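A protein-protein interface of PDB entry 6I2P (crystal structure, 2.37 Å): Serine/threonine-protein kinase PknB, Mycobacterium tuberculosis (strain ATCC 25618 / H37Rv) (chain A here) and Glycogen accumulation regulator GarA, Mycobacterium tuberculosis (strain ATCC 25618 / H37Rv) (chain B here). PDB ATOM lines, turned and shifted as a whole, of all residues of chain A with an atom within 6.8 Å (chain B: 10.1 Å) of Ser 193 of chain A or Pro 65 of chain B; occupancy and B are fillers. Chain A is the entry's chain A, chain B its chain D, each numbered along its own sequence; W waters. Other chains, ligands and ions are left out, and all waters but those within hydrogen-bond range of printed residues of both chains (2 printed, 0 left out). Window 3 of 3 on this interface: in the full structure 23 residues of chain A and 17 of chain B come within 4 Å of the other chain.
Of the 16 printed residues of chain B, 4 touch a printed residue of chain A.
Of chain B, only Pro 65 comes within 4 Å of Ser 193 of chain A. Of the printed residues of chain A, Pro 65 of chain B touches Ser 193. No residue of chain B comes within 4 Å of Glu 187 of chain A. Printed residues of chain B within 4 Å of Asp 192 of chain A: Arg 63. No residue of chain B comes within 4 Å of Val 194 of chain A. Of the printed residues of chain B, Gly 191 of chain A touches Leu 31 (3.7 Å) and Lys 142 (3.9 Å). Of the printed residues of chain B, Gln 188 of chain A touches Leu 31 (3.4 Å). Of the printed residues of chain A, Lys 142 of chain B touches Gly 191. Printed residues of chain A within 4 Å of Leu 31 of chain B: Gln 188 (3.4 Å) and Gly 191 (3.7 Å). Asp 92 of chain B touches none of the printed residues of chain A. Asn 66 of chain B touches none of the printed residues of chain A. The nearest residue of chain B that does not touch Ser 193 of chain A is Gly 64 of chain B (4.2 Å). The nearest residue of chain A that does not touch Pro 65 of chain B is Asp 192 of chain A (4.9 Å). The nearest printed residue of chain A that does not touch Leu 31 of chain B is Glu 187 of chain A (5.8 Å).
Water W1 bridges O of Lys 142 of chain B (2.6 Å) and O of Gly 191 of chain A (2.7 Å). Water W2 bridges NE2 of Gln 188 of chain A (3.2 Å) and NZ of Lys 142 of chain B (3.4 Å).
The side-chain hydroxyl (OG) of Ser 185 of chain A sits close to the backbone NH (N) of Gln 188 of chain A. The backbone NH of Asp 192 of chain A is in hydrogen-bond range of the backbone carbonyl oxygen of Glu 187 of chain A, at 2.8 Å. OD2 of Asp 92 of chain B lies within hydrogen-bond range of N of Lys 142 of chain B (2.7 Å).
Gln 188 of chain A touches Leu 31 of chain B. CD1 of Leu 31 of chain B touches CA of Gly 191 of chain A (3.7 Å). O of Lys 142 of chain B touches O of Gly 191 of chain A, 3.9 Å away. Asp 192 of chain A touches Arg 63 of chain B (OD1 to CD, 3.97 Å). CB of Ser 193 of chain A touches CG of Pro 65 of chain B (3.8 Å).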
ATOM      1  N   SER A 185     -29.052  -9.115   7.261  1.00  0.00           N
ATOM      2  CA  SER A 185     -28.370  -9.681   6.104  1.00  0.00           C
ATOM      3  C   SER A 185     -29.051 -11.027   5.778  1.00  0.00           C
ATOM      4  O   SER A 185     -29.681 -11.591   6.678  1.00  0.00           O
ATOM      5  CB  SER A 185     -26.890  -9.881   6.407  1.00  0.00           C
ATOM      6  OG  SER A 185     -26.704 -10.844   7.430  1.00  0.00           O
ATOM      7  N   GLU A 187     -27.854 -14.050   5.548  1.00  0.00           N
ATOM      8  CA  GLU A 187     -27.242 -15.047   6.441  1.00  0.00           C
ATOM      9  C   GLU A 187     -27.765 -14.977   7.881  1.00  0.00           C
ATOM     10  O   GLU A 187     -27.905 -16.017   8.525  1.00  0.00           O
ATOM     11  CB  GLU A 187     -25.690 -15.001   6.397  1.00  0.00           C
ATOM     12  CG  GLU A 187     -25.043 -13.662   6.743  1.00  0.00           C
ATOM     13  CD  GLU A 187     -24.767 -12.726   5.579  1.00  0.00           C
ATOM     14  OE1 GLU A 187     -25.549 -12.729   4.600  1.00  0.00           O
ATOM     15  OE2 GLU A 187     -23.768 -11.976   5.655  1.00  0.00           O
ATOM     16  N   GLN A 188     -28.062 -13.761   8.375  1.00  0.00           N
ATOM     17  CA  GLN A 188     -28.616 -13.534   9.715  1.00  0.00           C
ATOM     18  C   GLN A 188     -30.050 -14.042   9.798  1.00  0.00           C
ATOM     19  O   GLN A 188     -30.411 -14.685  10.782  1.00  0.00           O
ATOM     20  CB  GLN A 188     -28.575 -12.046  10.082  1.00  0.00           C
ATOM     21  CG  GLN A 188     -27.240 -11.595  10.649  1.00  0.00           C
ATOM     22  CD  GLN A 188     -27.274 -10.156  11.086  1.00  0.00           C
ATOM     23  OE1 GLN A 188     -27.831  -9.283  10.409  1.00  0.00           O
ATOM     24  NE2 GLN A 188     -26.671  -9.878  12.229  1.00  0.00           N
ATOM     25  N   GLY A 191     -29.852 -17.979   9.566  1.00  0.00           N
ATOM     26  CA  GLY A 191     -29.100 -18.660  10.617  1.00  0.00           C
ATOM     27  C   GLY A 191     -27.811 -19.269  10.084  1.00  0.00           C
ATOM     28  O   GLY A 191     -27.256 -20.197  10.684  1.00  0.00           O
ATOM     29  N   ASP A 192     -27.330 -18.753   8.935  1.00  0.00           N
ATOM     30  CA  ASP A 192     -26.077 -19.171   8.313  1.00  0.00           C
ATOM     31  C   ASP A 192     -24.917 -18.496   9.058  1.00  0.00           C
ATOM     32  O   ASP A 192     -25.159 -17.709   9.985  1.00  0.00           O
ATOM     33  CB  ASP A 192     -26.055 -18.774   6.821  1.00  0.00           C
ATOM     34  CG  ASP A 192     -26.944 -19.601   5.913  1.00  0.00           C
ATOM     35  OD1 ASP A 192     -26.898 -20.849   6.013  1.00  0.00           O
ATOM     36  OD2 ASP A 192     -27.660 -19.003   5.081  1.00  0.00           O
ATOM     37  N   SER A 193     -23.665 -18.798   8.661  1.00  0.00           N
ATOM     38  CA  SER A 193     -22.471 -18.195   9.272  1.00  0.00           C
ATOM     39  C   SER A 193     -22.463 -16.691   9.057  1.00  0.00           C
ATOM     40  O   SER A 193     -22.842 -16.218   7.984  1.00  0.00           O
ATOM     41  CB  SER A 193     -21.184 -18.802   8.715  1.00  0.00           C
ATOM     42  OG  SER A 193     -21.433 -19.765   7.705  1.00  0.00           O
ATOM     43  N   VAL A 194     -22.069 -15.948  10.088  1.00  0.00           N
ATOM     44  CA  VAL A 194     -22.017 -14.493  10.049  1.00  0.00           C
ATOM     45  C   VAL A 194     -20.576 -14.026  10.234  1.00  0.00           C
ATOM     46  O   VAL A 194     -19.908 -14.422  11.194  1.00  0.00           O
ATOM     47  CB  VAL A 194     -23.017 -13.851  11.066  1.00  0.00           C
ATOM     48  CG1 VAL A 194     -22.820 -12.343  11.200  1.00  0.00           C
ATOM     49  CG2 VAL A 194     -24.460 -14.161  10.681  1.00  0.00           C
ATOM     50  N   ASP A 195     -20.103 -13.205   9.285  1.00  0.00           N
ATOM     51  CA  ASP A 195     -18.779 -12.586   9.296  1.00  0.00           C
ATOM     52  C   ASP A 195     -18.931 -11.064   9.090  1.00  0.00           C
ATOM     53  O   ASP A 195     -20.060 -10.560   9.140  1.00  0.00           O
ATOM     54  CB  ASP A 195     -17.816 -13.266   8.297  1.00  0.00           C
ATOM     55  CG  ASP A 195     -18.274 -13.265   6.856  1.00  0.00           C
ATOM     56  OD1 ASP A 195     -18.172 -12.209   6.205  1.00  0.00           O
ATOM     57  OD2 ASP A 195     -18.720 -14.325   6.378  1.00  0.00           O
ATOM     58  N   SER A 198     -21.519  -9.140   6.728  1.00  0.00           N
ATOM     59  CA  SER A 198     -22.899  -8.983   7.177  1.00  0.00           C
ATOM     60  C   SER A 198     -23.101  -7.507   7.535  1.00  0.00           C
ATOM     61  O   SER A 198     -24.151  -6.936   7.231  1.00  0.00           O
ATOM     62  CB  SER A 198     -23.166  -9.878   8.379  1.00  0.00           C
ATOM     63  OG  SER A 198     -24.532  -9.859   8.751  1.00  0.00           O
ATOM     64  N   PRO A 260     -22.213 -13.310   0.114  1.00  0.00           N
ATOM     65  CA  PRO A 260     -21.193 -12.417   0.706  1.00  0.00           C
ATOM     66  C   PRO A 260     -19.910 -12.295  -0.126  1.00  0.00           C
ATOM     67  O   PRO A 260     -19.212 -11.287  -0.041  1.00  0.00           O
ATOM     68  CB  PRO A 260     -20.933 -13.041   2.084  1.00  0.00           C
ATOM     69  CG  PRO A 260     -22.145 -13.859   2.374  1.00  0.00           C
ATOM     70  CD  PRO A 260     -22.564 -14.402   1.045  1.00  0.00           C
ATOM     71  N   LEU B  31     -34.971 -18.168  10.903  1.00  0.00           N
ATOM     72  CA  LEU B  31     -34.901 -18.417  12.346  1.00  0.00           C
ATOM     73  C   LEU B  31     -36.259 -18.063  12.965  1.00  0.00           C
ATOM     74  O   LEU B  31     -36.953 -17.173  12.466  1.00  0.00           O
ATOM     75  CB  LEU B  31     -33.762 -17.618  13.014  1.00  0.00           C
ATOM     76  CG  LEU B  31     -32.321 -18.057  12.685  1.00  0.00           C
ATOM     77  CD1 LEU B  31     -31.334 -17.012  13.121  1.00  0.00           C
ATOM     78  CD2 LEU B  31     -31.964 -19.391  13.342  1.00  0.00           C
ATOM     79  N   VAL B  61     -26.733 -30.882  13.476  1.00  0.00           N
ATOM     80  CA  VAL B  61     -26.742 -29.463  13.112  1.00  0.00           C
ATOM     81  C   VAL B  61     -27.047 -29.418  11.601  1.00  0.00           C
ATOM     82  O   VAL B  61     -26.313 -30.001  10.799  1.00  0.00           O
ATOM     83  CB  VAL B  61     -25.434 -28.711  13.485  1.00  0.00           C
ATOM     84  CG1 VAL B  61     -25.594 -27.206  13.291  1.00  0.00           C
ATOM     85  CG2 VAL B  61     -25.003 -29.015  14.914  1.00  0.00           C
ATOM     86  N   LYS B  62     -28.165 -28.775  11.238  1.00  0.00           N
ATOM     87  CA  LYS B  62     -28.637 -28.685   9.858  1.00  0.00           C
ATOM     88  C   LYS B  62     -27.867 -27.681   8.993  1.00  0.00           C
ATOM     89  O   LYS B  62     -27.608 -27.974   7.827  1.00  0.00           O
ATOM     90  CB  LYS B  62     -30.142 -28.380   9.836  1.00  0.00           C
ATOM     91  CG  LYS B  62     -30.921 -29.228   8.849  1.00  0.00           C
ATOM     92  CD  LYS B  62     -32.325 -28.689   8.622  1.00  0.00           C
ATOM     93  CE  LYS B  62     -33.153 -29.670   7.826  1.00  0.00           C
ATOM     94  NZ  LYS B  62     -34.454 -29.090   7.413  1.00  0.00           N
ATOM     95  N   ARG B  63     -27.517 -26.501   9.542  1.00  0.00           N
ATOM     96  CA  ARG B  63     -26.815 -25.454   8.787  1.00  0.00           C
ATOM     97  C   ARG B  63     -25.820 -24.632   9.622  1.00  0.00           C
ATOM     98  O   ARG B  63     -25.769 -24.762  10.844  1.00  0.00           O
ATOM     99  CB  ARG B  63     -27.809 -24.532   8.046  1.00  0.00           C
ATOM    100  CG  ARG B  63     -28.810 -23.797   8.936  1.00  0.00           C
ATOM    101  CD  ARG B  63     -29.626 -22.780   8.152  1.00  0.00           C
ATOM    102  NE  ARG B  63     -30.643 -23.428   7.328  1.00  0.00           N
ATOM    103  CZ  ARG B  63     -31.625 -22.793   6.697  1.00  0.00           C
ATOM    104  NH1 ARG B  63     -32.504 -23.474   5.977  1.00  0.00           N
ATOM    105  NH2 ARG B  63     -31.740 -21.474   6.788  1.00  0.00           N
ATOM    106  N   GLY B  64     -25.040 -23.797   8.936  1.00  0.00           N
ATOM    107  CA  GLY B  64     -24.061 -22.897   9.541  1.00  0.00           C
ATOM    108  C   GLY B  64     -22.650 -23.450   9.612  1.00  0.00           C
ATOM    109  O   GLY B  64     -22.331 -24.414   8.908  1.00  0.00           O
ATOM    110  N   PRO B  65     -21.782 -22.863  10.477  1.00  0.00           N
ATOM    111  CA  PRO B  65     -20.389 -23.348  10.586  1.00  0.00           C
ATOM    112  C   PRO B  65     -20.239 -24.783  11.090  1.00  0.00           C
ATOM    113  O   PRO B  65     -19.292 -25.464  10.712  1.00  0.00           O
ATOM    114  CB  PRO B  65     -19.739 -22.362  11.569  1.00  0.00           C
ATOM    115  CG  PRO B  65     -20.640 -21.197  11.621  1.00  0.00           C
ATOM    116  CD  PRO B  65     -22.014 -21.710  11.371  1.00  0.00           C
ATOM    117  N   ASN B  66     -21.157 -25.232  11.949  1.00  0.00           N
ATOM    118  CA  ASN B  66     -21.131 -26.572  12.532  1.00  0.00           C
ATOM    119  C   ASN B  66     -22.039 -27.580  11.812  1.00  0.00           C
ATOM    120  O   ASN B  66     -22.250 -28.668  12.339  1.00  0.00           O
ATOM    121  CB  ASN B  66     -21.449 -26.500  14.034  1.00  0.00           C
ATOM    122  CG  ASN B  66     -20.468 -25.652  14.795  1.00  0.00           C
ATOM    123  OD1 ASN B  66     -19.314 -26.037  15.027  1.00  0.00           O
ATOM    124  ND2 ASN B  66     -20.903 -24.465  15.177  1.00  0.00           N
ATOM    125  N   ALA B  67     -22.557 -27.236  10.606  1.00  0.00           N
ATOM    126  CA  ALA B  67     -23.429 -28.117   9.818  1.00  0.00           C
ATOM    127  C   ALA B  67     -22.770 -29.475   9.634  1.00  0.00           C
ATOM    128  O   ALA B  67     -21.613 -29.544   9.214  1.00  0.00           O
ATOM    129  CB  ALA B  67     -23.728 -27.500   8.462  1.00  0.00           C
ATOM    130  N   GLY B  68     -23.491 -30.530   9.999  1.00  0.00           N
ATOM    131  CA  GLY B  68     -22.992 -31.894   9.901  1.00  0.00           C
ATOM    132  C   GLY B  68     -22.610 -32.481  11.242  1.00  0.00           C
ATOM    133  O   GLY B  68     -22.609 -33.705  11.391  1.00  0.00           O
ATOM    134  N   SER B  69     -22.292 -31.609  12.233  1.00  0.00           N
ATOM    135  CA  SER B  69     -21.956 -32.028  13.595  1.00  0.00           C
ATOM    136  C   SER B  69     -23.178 -32.658  14.228  1.00  0.00           C
ATOM    137  O   SER B  69     -24.304 -32.231  13.977  1.00  0.00           O
ATOM    138  CB  SER B  69     -21.476 -30.856  14.447  1.00  0.00           C
ATOM    139  OG  SER B  69     -20.169 -30.464  14.062  1.00  0.00           O
ATOM    140  N   ARG B  70     -22.957 -33.710  14.998  1.00  0.00           N
ATOM    141  CA  ARG B  70     -24.042 -34.440  15.628  1.00  0.00           C
ATOM    142  C   ARG B  70     -23.729 -34.818  17.057  1.00  0.00           C
ATOM    143  O   ARG B  70     -22.570 -34.817  17.469  1.00  0.00           O
ATOM    144  CB  ARG B  70     -24.476 -35.659  14.783  1.00  0.00           C
ATOM    145  CG  ARG B  70     -23.363 -36.652  14.465  1.00  0.00           C
ATOM    146  CD  ARG B  70     -23.637 -37.392  13.171  1.00  0.00           C
ATOM    147  NE  ARG B  70     -23.624 -36.472  12.033  1.00  0.00           N
ATOM    148  CZ  ARG B  70     -24.344 -36.623  10.928  1.00  0.00           C
ATOM    149  NH1 ARG B  70     -25.134 -37.679  10.780  1.00  0.00           N
ATOM    150  NH2 ARG B  70     -24.271 -35.728   9.956  1.00  0.00           N
ATOM    151  N   ASP B  91     -21.249 -23.550  21.019  1.00  0.00           N
ATOM    152  CA  ASP B  91     -20.528 -22.286  21.053  1.00  0.00           C
ATOM    153  C   ASP B  91     -21.112 -21.284  20.072  1.00  0.00           C
ATOM    154  O   ASP B  91     -20.836 -21.330  18.871  1.00  0.00           O
ATOM    155  CB  ASP B  91     -19.024 -22.505  20.818  1.00  0.00           C
ATOM    156  CG  ASP B  91     -18.140 -21.326  21.188  1.00  0.00           C
ATOM    157  OD1 ASP B  91     -18.599 -20.454  21.970  1.00  0.00           O
ATOM    158  OD2 ASP B  91     -16.988 -21.278  20.706  1.00  0.00           O
ATOM    159  N   ASP B  92     -21.928 -20.372  20.603  1.00  0.00           N
ATOM    160  CA  ASP B  92     -22.624 -19.304  19.890  1.00  0.00           C
ATOM    161  C   ASP B  92     -23.011 -18.259  20.945  1.00  0.00           C
ATOM    162  O   ASP B  92     -23.537 -18.641  21.987  1.00  0.00           O
ATOM    163  CB  ASP B  92     -23.854 -19.917  19.192  1.00  0.00           C
ATOM    164  CG  ASP B  92     -24.983 -19.031  18.701  1.00  0.00           C
ATOM    165  OD1 ASP B  92     -24.982 -17.817  19.018  1.00  0.00           O
ATOM    166  OD2 ASP B  92     -25.877 -19.553  18.027  1.00  0.00           O
ATOM    167  N   LYS B 142     -28.545 -19.821  17.494  1.00  0.00           N
ATOM    168  CA  LYS B 142     -28.559 -19.791  16.034  1.00  0.00           C
ATOM    169  C   LYS B 142     -28.409 -21.225  15.495  1.00  0.00           C
ATOM    170  O   LYS B 142     -28.299 -21.409  14.283  1.00  0.00           O
ATOM    171  CB  LYS B 142     -27.448 -18.874  15.477  1.00  0.00           C
ATOM    172  CG  LYS B 142     -27.648 -17.388  15.734  1.00  0.00           C
ATOM    173  CD  LYS B 142     -26.525 -16.585  15.087  1.00  0.00           C
ATOM    174  CE  LYS B 142     -25.674 -15.839  16.089  1.00  0.00           C
ATOM    175  NZ  LYS B 142     -24.488 -15.222  15.448  1.00  0.00           N
ATOM    176  N   PHE B 143     -28.391 -22.238  16.390  1.00  0.00           N
ATOM    177  CA  PHE B 143     -28.280 -23.644  15.993  1.00  0.00           C
ATOM    178  C   PHE B 143     -29.640 -24.212  15.626  1.00  0.00           C
ATOM    179  O   PHE B 143     -30.598 -24.066  16.378  1.00  0.00           O
ATOM    180  CB  PHE B 143     -27.652 -24.507  17.101  1.00  0.00           C
ATOM    181  CG  PHE B 143     -26.165 -24.342  17.282  1.00  0.00           C
ATOM    182  CD1 PHE B 143     -25.658 -23.411  18.182  1.00  0.00           C
ATOM    183  CD2 PHE B 143     -25.266 -25.139  16.575  1.00  0.00           C
ATOM    184  CE1 PHE B 143     -24.279 -23.272  18.367  1.00  0.00           C
ATOM    185  CE2 PHE B 143     -23.883 -24.989  16.750  1.00  0.00           C
ATOM    186  CZ  PHE B 143     -23.401 -24.061  17.652  1.00  0.00           C
ATOM    187  N   ARG B 144     -29.717 -24.857  14.465  1.00  0.00           N
ATOM    188  CA  ARG B 144     -30.916 -25.519  13.966  1.00  0.00           C
ATOM    189  C   ARG B 144     -30.588 -27.001  13.939  1.00  0.00           C
ATOM    190  O   ARG B 144     -29.884 -27.486  13.050  1.00  0.00           O
ATOM    191  CB  ARG B 144     -31.329 -24.967  12.591  1.00  0.00           C
ATOM    192  CG  ARG B 144     -32.023 -23.601  12.682  1.00  0.00           C
ATOM    193  CD  ARG B 144     -32.226 -22.956  11.323  1.00  0.00           C
ATOM    194  NE  ARG B 144     -33.053 -23.780  10.437  1.00  0.00           N
ATOM    195  CZ  ARG B 144     -34.058 -23.321   9.699  1.00  0.00           C
ATOM    196  NH1 ARG B 144     -34.381 -22.036   9.730  1.00  0.00           N
ATOM    197  NH2 ARG B 144     -34.745 -24.144   8.919  1.00  0.00           N
HETATM  198  O   HOH W   1     -28.839 -22.113  11.801  1.00  0.00           O
HETATM  199  O   HOH W   2     -25.513 -12.256  14.038  1.00  0.00           O
